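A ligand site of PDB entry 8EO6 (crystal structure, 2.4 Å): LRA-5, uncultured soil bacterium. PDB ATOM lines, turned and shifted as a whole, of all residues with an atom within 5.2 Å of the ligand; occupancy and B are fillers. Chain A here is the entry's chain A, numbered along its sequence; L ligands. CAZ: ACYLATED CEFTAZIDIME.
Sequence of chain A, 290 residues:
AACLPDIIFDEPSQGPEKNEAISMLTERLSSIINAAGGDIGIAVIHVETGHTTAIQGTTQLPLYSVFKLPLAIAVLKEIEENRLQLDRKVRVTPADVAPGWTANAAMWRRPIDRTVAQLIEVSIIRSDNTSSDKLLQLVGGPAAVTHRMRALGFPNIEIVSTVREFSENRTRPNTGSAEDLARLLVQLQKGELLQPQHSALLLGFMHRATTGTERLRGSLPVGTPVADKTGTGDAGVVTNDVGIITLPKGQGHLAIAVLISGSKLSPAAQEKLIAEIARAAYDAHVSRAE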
ATOM      1  N   TYR A  64      -8.724  -7.602   5.215  1.00  0.00           N
ATOM      2  CA  TYR A  64      -7.252  -7.699   5.112  1.00  0.00           C
ATOM      3  C   TYR A  64      -6.933  -8.525   3.864  1.00  0.00           C
ATOM      4  O   TYR A  64      -7.483  -8.236   2.797  1.00  0.00           O
ATOM      5  CB  TYR A  64      -6.682  -8.218   6.424  1.00  0.00           C
ATOM      6  CG  TYR A  64      -6.637  -7.171   7.521  1.00  0.00           C
ATOM      7  CD1 TYR A  64      -7.808  -6.551   7.968  1.00  0.00           C
ATOM      8  CD2 TYR A  64      -5.441  -6.799   8.114  1.00  0.00           C
ATOM      9  CE1 TYR A  64      -7.767  -5.597   8.973  1.00  0.00           C
ATOM     10  CE2 TYR A  64      -5.396  -5.839   9.106  1.00  0.00           C
ATOM     11  CZ  TYR A  64      -6.562  -5.244   9.536  1.00  0.00           C
ATOM     12  OH  TYR A  64      -6.506  -4.289  10.522  1.00  0.00           O
ATOM     13  N   SER A  65      -6.095  -9.550   3.950  1.00  0.00           N
ATOM     14  CA  SER A  65      -5.656 -10.247   2.743  1.00  0.00           C
ATOM     15  C   SER A  65      -6.740 -11.110   2.104  1.00  0.00           C
ATOM     16  O   SER A  65      -6.508 -11.666   1.022  1.00  0.00           O
ATOM     17  CB  SER A  65      -4.441 -11.114   3.043  1.00  0.00           C
ATOM     18  OG  SER A  65      -3.297 -10.312   3.261  1.00  0.00           O
ATOM     19  N   VAL A  66      -7.903 -11.274   2.743  1.00  0.00           N
ATOM     20  CA  VAL A  66      -8.992 -12.019   2.115  1.00  0.00           C
ATOM     21  C   VAL A  66      -9.468 -11.308   0.857  1.00  0.00           C
ATOM     22  O   VAL A  66      -9.957 -11.948  -0.091  1.00  0.00           O
ATOM     23  CB  VAL A  66     -10.133 -12.248   3.138  1.00  0.00           C
ATOM     24  CG1 VAL A  66     -11.462 -12.547   2.452  1.00  0.00           C
ATOM     25  CG2 VAL A  66      -9.763 -13.378   4.074  1.00  0.00           C
ATOM     26  N   LYS A  68      -7.833 -10.359  -1.501  1.00  0.00           N
ATOM     27  CA  LYS A  68      -7.117 -10.839  -2.671  1.00  0.00           C
ATOM     28  C   LYS A  68      -7.926 -11.856  -3.458  1.00  0.00           C
ATOM     29  O   LYS A  68      -7.642 -12.085  -4.635  1.00  0.00           O
ATOM     30  CB  LYS A  68      -5.776 -11.463  -2.268  1.00  0.00           C
ATOM     31  CG  LYS A  68      -4.777 -10.504  -1.606  1.00  0.00           C
ATOM     32  CD  LYS A  68      -3.585 -11.278  -1.077  1.00  0.00           C
ATOM     33  CE  LYS A  68      -2.414 -10.383  -0.710  1.00  0.00           C
ATOM     34  NZ  LYS A  68      -2.742  -9.459   0.401  1.00  0.00           N
ATOM     35  N   ALA A 103       7.460  -9.605   4.264  1.00  0.00           N
ATOM     36  CA  ALA A 103       7.278 -11.061   4.178  1.00  0.00           C
ATOM     37  C   ALA A 103       7.815 -11.633   2.866  1.00  0.00           C
ATOM     38  O   ALA A 103       8.649 -12.545   2.871  1.00  0.00           O
ATOM     39  CB  ALA A 103       5.796 -11.400   4.348  1.00  0.00           C
ATOM     40  N   ASN A 104       7.360 -11.102   1.737  1.00  0.00           N
ATOM     41  CA  ASN A 104       7.672 -11.667   0.434  1.00  0.00           C
ATOM     42  C   ASN A 104       8.590 -10.792  -0.429  1.00  0.00           C
ATOM     43  O   ASN A 104       8.726 -11.053  -1.629  1.00  0.00           O
ATOM     44  CB  ASN A 104       6.378 -11.959  -0.335  1.00  0.00           C
ATOM     45  CG  ASN A 104       5.438 -12.890   0.406  1.00  0.00           C
ATOM     46  OD1 ASN A 104       5.484 -14.113   0.226  1.00  0.00           O
ATOM     47  ND2 ASN A 104       4.560 -12.331   1.241  1.00  0.00           N
ATOM     48  N   ARG A 126       1.060 -16.855  -1.587  1.00  0.00           N
ATOM     49  CA  ARG A 126       1.930 -16.245  -0.582  1.00  0.00           C
ATOM     50  C   ARG A 126       1.308 -15.032   0.091  1.00  0.00           C
ATOM     51  O   ARG A 126       1.970 -14.434   0.948  1.00  0.00           O
ATOM     52  CB  ARG A 126       3.263 -15.845  -1.220  1.00  0.00           C
ATOM     53  CG  ARG A 126       4.029 -16.992  -1.839  1.00  0.00           C
ATOM     54  CD  ARG A 126       4.780 -17.784  -0.785  1.00  0.00           C
ATOM     55  NE  ARG A 126       6.095 -18.219  -1.271  1.00  0.00           N
ATOM     56  CZ  ARG A 126       6.390 -19.465  -1.622  1.00  0.00           C
ATOM     57  NH1 ARG A 126       5.480 -20.430  -1.576  1.00  0.00           N
ATOM     58  NH2 ARG A 126       7.615 -19.739  -2.049  1.00  0.00           N
ATOM     59  N   SER A 127       0.073 -14.670  -0.249  1.00  0.00           N
ATOM     60  CA  SER A 127      -0.560 -13.472   0.291  1.00  0.00           C
ATOM     61  C   SER A 127       0.322 -12.249   0.077  1.00  0.00           C
ATOM     62  O   SER A 127       0.518 -11.423   0.962  1.00  0.00           O
ATOM     63  CB  SER A 127      -0.923 -13.652   1.776  1.00  0.00           C
ATOM     64  OG  SER A 127      -2.093 -12.929   2.116  1.00  0.00           O
ATOM     65  N   ASN A 129       1.562  -8.730  -0.919  1.00  0.00           N
ATOM     66  CA  ASN A 129       0.977  -7.396  -1.031  1.00  0.00           C
ATOM     67  C   ASN A 129       1.429  -6.680  -2.301  1.00  0.00           C
ATOM     68  O   ASN A 129       0.635  -5.949  -2.918  1.00  0.00           O
ATOM     69  CB  ASN A 129       1.336  -6.564   0.203  1.00  0.00           C
ATOM     70  CG  ASN A 129       0.667  -7.062   1.458  1.00  0.00           C
ATOM     71  OD1 ASN A 129      -0.371  -7.726   1.402  1.00  0.00           O
ATOM     72  ND2 ASN A 129       1.255  -6.753   2.606  1.00  0.00           N
ATOM     73  N   VAL A 163      -3.488  -1.794  -0.807  1.00  0.00           N
ATOM     74  CA  VAL A 163      -2.778  -2.375   0.336  1.00  0.00           C
ATOM     75  C   VAL A 163      -1.843  -1.353   0.974  1.00  0.00           C
ATOM     76  O   VAL A 163      -1.733  -1.283   2.203  1.00  0.00           O
ATOM     77  CB  VAL A 163      -2.021  -3.644  -0.097  1.00  0.00           C
ATOM     78  CG1 VAL A 163      -1.421  -4.330   1.117  1.00  0.00           C
ATOM     79  CG2 VAL A 163      -2.933  -4.595  -0.857  1.00  0.00           C
ATOM     80  N   PHE A 166      -3.885   1.373   2.982  1.00  0.00           N
ATOM     81  CA  PHE A 166      -4.364   0.836   4.250  1.00  0.00           C
ATOM     82  C   PHE A 166      -3.220   0.585   5.226  1.00  0.00           C
ATOM     83  O   PHE A 166      -3.435   0.611   6.448  1.00  0.00           O
ATOM     84  CB  PHE A 166      -5.129  -0.472   4.011  1.00  0.00           C
ATOM     85  CG  PHE A 166      -5.669  -1.083   5.274  1.00  0.00           C
ATOM     86  CD1 PHE A 166      -6.521  -0.368   6.099  1.00  0.00           C
ATOM     87  CD2 PHE A 166      -5.299  -2.367   5.645  1.00  0.00           C
ATOM     88  CE1 PHE A 166      -7.006  -0.928   7.265  1.00  0.00           C
ATOM     89  CE2 PHE A 166      -5.782  -2.936   6.808  1.00  0.00           C
ATOM     90  CZ  PHE A 166      -6.642  -2.218   7.616  1.00  0.00           C
ATOM     91  N   SER A 167      -2.016   0.339   4.723  1.00  0.00           N
ATOM     92  CA  SER A 167      -0.883   0.051   5.597  1.00  0.00           C
ATOM     93  C   SER A 167      -0.388   1.286   6.338  1.00  0.00           C
ATOM     94  O   SER A 167       0.125   1.158   7.450  1.00  0.00           O
ATOM     95  CB  SER A 167       0.257  -0.567   4.783  1.00  0.00           C
ATOM     96  OG  SER A 167       1.238   0.399   4.477  1.00  0.00           O
ATOM     97  N   ARG A 170      -4.649   2.392   9.515  1.00  0.00           N
ATOM     98  CA  ARG A 170      -5.743   1.419   9.593  1.00  0.00           C
ATOM     99  C   ARG A 170      -6.986   2.176  10.054  1.00  0.00           C
ATOM    100  O   ARG A 170      -7.236   2.413  11.238  1.00  0.00           O
ATOM    101  CB  ARG A 170      -5.373   0.219  10.473  1.00  0.00           C
ATOM    102  CG  ARG A 170      -5.526   0.337  11.984  1.00  0.00           C
ATOM    103  CD  ARG A 170      -4.309  -0.180  12.734  1.00  0.00           C
ATOM    104  NE  ARG A 170      -4.300   0.234  14.125  1.00  0.00           N
ATOM    105  CZ  ARG A 170      -4.096   1.471  14.558  1.00  0.00           C
ATOM    106  NH1 ARG A 170      -3.877   2.462  13.716  1.00  0.00           N
ATOM    107  NH2 ARG A 170      -4.113   1.725  15.867  1.00  0.00           N
ATOM    108  N   THR A 211      -0.455 -20.072   3.753  1.00  0.00           N
ATOM    109  CA  THR A 211      -0.542 -19.176   4.900  1.00  0.00           C
ATOM    110  C   THR A 211      -1.579 -19.608   5.939  1.00  0.00           C
ATOM    111  O   THR A 211      -1.653 -18.980   7.002  1.00  0.00           O
ATOM    112  CB  THR A 211      -0.849 -17.746   4.421  1.00  0.00           C
ATOM    113  OG1 THR A 211      -2.116 -17.710   3.762  1.00  0.00           O
ATOM    114  CG2 THR A 211       0.236 -17.263   3.445  1.00  0.00           C
ATOM    115  N   ARG A 215      -5.559 -22.967  10.138  1.00  0.00           N
ATOM    116  CA  ARG A 215      -6.922 -22.434  10.182  1.00  0.00           C
ATOM    117  C   ARG A 215      -7.919 -23.452   9.631  1.00  0.00           C
ATOM    118  O   ARG A 215      -8.188 -24.459  10.303  1.00  0.00           O
ATOM    119  CB  ARG A 215      -6.969 -21.094   9.449  1.00  0.00           C
ATOM    120  CG  ARG A 215      -6.107 -20.041  10.149  1.00  0.00           C
ATOM    121  CD  ARG A 215      -6.100 -18.682   9.484  1.00  0.00           C
ATOM    122  NE  ARG A 215      -4.938 -17.897   9.903  1.00  0.00           N
ATOM    123  CZ  ARG A 215      -4.808 -16.595   9.765  1.00  0.00           C
ATOM    124  NH1 ARG A 215      -5.751 -15.855   9.199  1.00  0.00           N
ATOM    125  NH2 ARG A 215      -3.708 -15.997  10.217  1.00  0.00           N
ATOM    126  N   THR A 230      -6.383 -16.727   3.425  1.00  0.00           N
ATOM    127  CA  THR A 230      -6.379 -16.227   4.788  1.00  0.00           C
ATOM    128  C   THR A 230      -6.275 -14.703   4.822  1.00  0.00           C
ATOM    129  O   THR A 230      -5.966 -14.050   3.825  1.00  0.00           O
ATOM    130  CB  THR A 230      -5.235 -16.843   5.591  1.00  0.00           C
ATOM    131  OG1 THR A 230      -3.984 -16.500   4.972  1.00  0.00           O
ATOM    132  CG2 THR A 230      -5.381 -18.356   5.613  1.00  0.00           C
ATOM    133  N   GLY A 231      -6.561 -14.153   5.997  1.00  0.00           N
ATOM    134  CA  GLY A 231      -6.327 -12.743   6.275  1.00  0.00           C
ATOM    135  C   GLY A 231      -5.850 -12.563   7.692  1.00  0.00           C
ATOM    136  O   GLY A 231      -6.454 -13.098   8.627  1.00  0.00           O
ATOM    137  N   THR A 232      -4.765 -11.807   7.886  1.00  0.00           N
ATOM    138  CA  THR A 232      -4.177 -11.623   9.205  1.00  0.00           C
ATOM    139  C   THR A 232      -3.726 -10.182   9.383  1.00  0.00           C
ATOM    140  O   THR A 232      -3.013  -9.651   8.539  1.00  0.00           O
ATOM    141  CB  THR A 232      -2.977 -12.562   9.410  1.00  0.00           C
ATOM    142  OG1 THR A 232      -3.221 -13.813   8.747  1.00  0.00           O
ATOM    143  CG2 THR A 232      -2.748 -12.815  10.898  1.00  0.00           C
ATOM    144  N   GLY A 233      -4.153  -9.569  10.490  1.00  0.00           N
ATOM    145  CA  GLY A 233      -3.566  -8.327  10.940  1.00  0.00           C
ATOM    146  C   GLY A 233      -2.566  -8.599  12.061  1.00  0.00           C
ATOM    147  O   GLY A 233      -2.642  -9.608  12.739  1.00  0.00           O
ATOM    148  N   ASP A 234      -1.615  -7.682  12.234  1.00  0.00           N
ATOM    149  CA  ASP A 234      -0.595  -7.881  13.257  1.00  0.00           C
ATOM    150  C   ASP A 234      -1.188  -7.765  14.644  1.00  0.00           C
ATOM    151  O   ASP A 234      -2.114  -6.976  14.877  1.00  0.00           O
ATOM    152  CB  ASP A 234       0.559  -6.890  13.085  1.00  0.00           C
ATOM    153  CG  ASP A 234       0.092  -5.480  12.771  1.00  0.00           C
ATOM    154  OD1 ASP A 234       0.501  -4.547  13.492  1.00  0.00           O
ATOM    155  OD2 ASP A 234      -0.681  -5.303  11.805  1.00  0.00           O
ATOM    156  N   VAL A 237      -5.250  -8.555  15.701  1.00  0.00           N
ATOM    157  CA  VAL A 237      -6.380  -7.659  15.500  1.00  0.00           C
ATOM    158  C   VAL A 237      -7.412  -8.284  14.571  1.00  0.00           C
ATOM    159  O   VAL A 237      -8.621  -8.070  14.733  1.00  0.00           O
ATOM    160  CB  VAL A 237      -5.886  -6.288  14.970  1.00  0.00           C
ATOM    161  CG1 VAL A 237      -4.980  -6.465  13.758  1.00  0.00           C
ATOM    162  CG2 VAL A 237      -7.056  -5.364  14.647  1.00  0.00           C
HETATM  163  S1  CAZ L   1       1.031  -9.939   4.288  1.00  0.00           S
HETATM  164  C2  CAZ L   1       1.958 -11.474   4.099  1.00  0.00           C
HETATM  165  C3  CAZ L   1       1.412 -12.665   4.830  1.00  0.00           C
HETATM  166  C3' CAZ L   1       2.192 -13.756   4.753  1.00  0.00           C
HETATM  167  C4  CAZ L   1       0.120 -12.614   5.556  1.00  0.00           C
HETATM  168  C4' CAZ L   1      -0.324 -13.847   6.489  1.00  0.00           C
HETATM  169  O4A CAZ L   1       0.597 -14.432   7.069  1.00  0.00           O
HETATM  170  O4B CAZ L   1      -1.545 -14.089   6.571  1.00  0.00           O
HETATM  171  N5  CAZ L   1      -0.820 -11.759   5.279  1.00  0.00           N
HETATM  172  C6  CAZ L   1      -0.647 -10.649   4.435  1.00  0.00           C
HETATM  173  C7  CAZ L   1      -1.632  -9.514   4.731  1.00  0.00           C
HETATM  174  C8  CAZ L   1      -3.032 -10.058   4.568  1.00  0.00           C
HETATM  175  O9  CAZ L   1      -3.797 -10.190   5.526  1.00  0.00           O
HETATM  176  N10 CAZ L   1      -1.418  -8.927   6.017  1.00  0.00           N
HETATM  177  C11 CAZ L   1      -0.701  -7.808   6.204  1.00  0.00           C
HETATM  178  O12 CAZ L   1      -0.176  -7.181   5.243  1.00  0.00           O
HETATM  179  C13 CAZ L   1      -0.552  -7.389   7.595  1.00  0.00           C
HETATM  180  N16 CAZ L   1       0.207  -8.036   8.490  1.00  0.00           N
HETATM  181  O17 CAZ L   1       0.848  -9.129   8.008  1.00  0.00           O
HETATM  182  C18 CAZ L   1       1.609  -9.902   9.050  1.00  0.00           C
HETATM  183  C14 CAZ L   1      -1.289  -6.184   7.974  1.00  0.00           C
HETATM  184  C15 CAZ L   1      -1.716  -5.230   7.069  1.00  0.00           C
HETATM  185  S16 CAZ L   1      -2.550  -3.920   7.828  1.00  0.00           S
HETATM  186  C17 CAZ L   1      -2.290  -4.741   9.386  1.00  0.00           C
HETATM  187  N18 CAZ L   1      -2.797  -4.124  10.533  1.00  0.00           N
HETATM  188  N19 CAZ L   1      -1.633  -5.888   9.315  1.00  0.00           N
HETATM  189  C19 CAZ L   1       2.571 -10.873   8.308  1.00  0.00           C
HETATM  190  C20 CAZ L   1       0.652 -10.747   9.880  1.00  0.00           C
HETATM  191  C21 CAZ L   1       2.527  -8.949   9.942  1.00  0.00           C
HETATM  192  O2A CAZ L   1       2.760  -9.335  11.103  1.00  0.00           O
HETATM  193  O2B CAZ L   1       2.945  -7.899   9.396  1.00  0.00           O
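N of Ser 65 sits close to O9 of the ligand. The side-chain hydroxyl of Ser 65 is covalently linked to a carbon (C8) of the ligand (1.4 Å). N of Asp 234 is in hydrogen-bond range of N19 of the ligand (3.4 Å). OD2 of Asp 234 sits at hydrogen-bond distance from N19 of the ligand (2.7 Å). The backbone NH of Thr 232 sits at hydrogen-bond distance from an oxygen (O9) of the ligand, 3.0 Å away. The backbone carbonyl oxygen (O) of Thr 232 lies within hydrogen-bond range of a nitrogen (N10) of the ligand (3.1 Å). The side-chain hydroxyl (OG1) of Thr 232 lies within hydrogen-bond range of an oxygen (O4B) of the ligand, 2.8 Å away. O12 of the ligand lies within hydrogen-bond range of ND2 of Asn 129, at 3.0 Å.
OG of Ser 65 is in hydrogen-bond range of OG of Ser 127, 3.1 Å away. The side-chain hydroxyl of Ser 65 sits at hydrogen-bond distance from the side-chain amino group of Lys 68, 3.0 Å away. The side-chain hydroxyl of Thr 232 is in hydrogen-bond range of the guanidinium group of Arg 215 (2.7 Å). OD1 of Asn 129 is in hydrogen-bond range of NZ of Lys 68, at 3.1 Å. The backbone carbonyl oxygen (O) of Gly 231 lies within hydrogen-bond range of the guanidinium group (NH1) of Arg 215 (2.9 Å). The side-chain hydroxyl (OG1) of Thr 230 lies within hydrogen-bond range of the side-chain hydroxyl (OG1) of Thr 211 (2.5 Å). O of Arg 126 lies within hydrogen-bond range of ND2 of Asn 104 (3.3 Å).
The backbone carbonyl oxygen of Ser 127 sits close to a sulfur (S1) of the ligand (3.7 Å). CE2 of Tyr 64 touches C17 of the ligand, at 3.3 Å. CB of Ala 103 touches C2 of the ligand, at 3.8 Å. ND2 of Asn 104 touches C2 of the ligand, 3.96 Å away. Arg 126 touches the ligand. Phe 166 touches the ligand (CE2 to S16, 3.5 Å). OG1 of Thr 230 touches O4B of the ligand (3.8 Å). Gly 231 touches the ligand. Gly 233 touches the ligand (CA to N19, 3.5 Å). Hydrophobic or aromatic side chains that line the ligand: Tyr 64, Ala 103 and Phe 166. 13 residues have an atom within 4 Å of the ligand: Tyr 64, Ser 65, Ala 103, Asn 104, Arg 126, Ser 127, Asn 129, Phe 166, Thr 230, Gly 231, Thr 232, Gly 233 and Asp 234.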
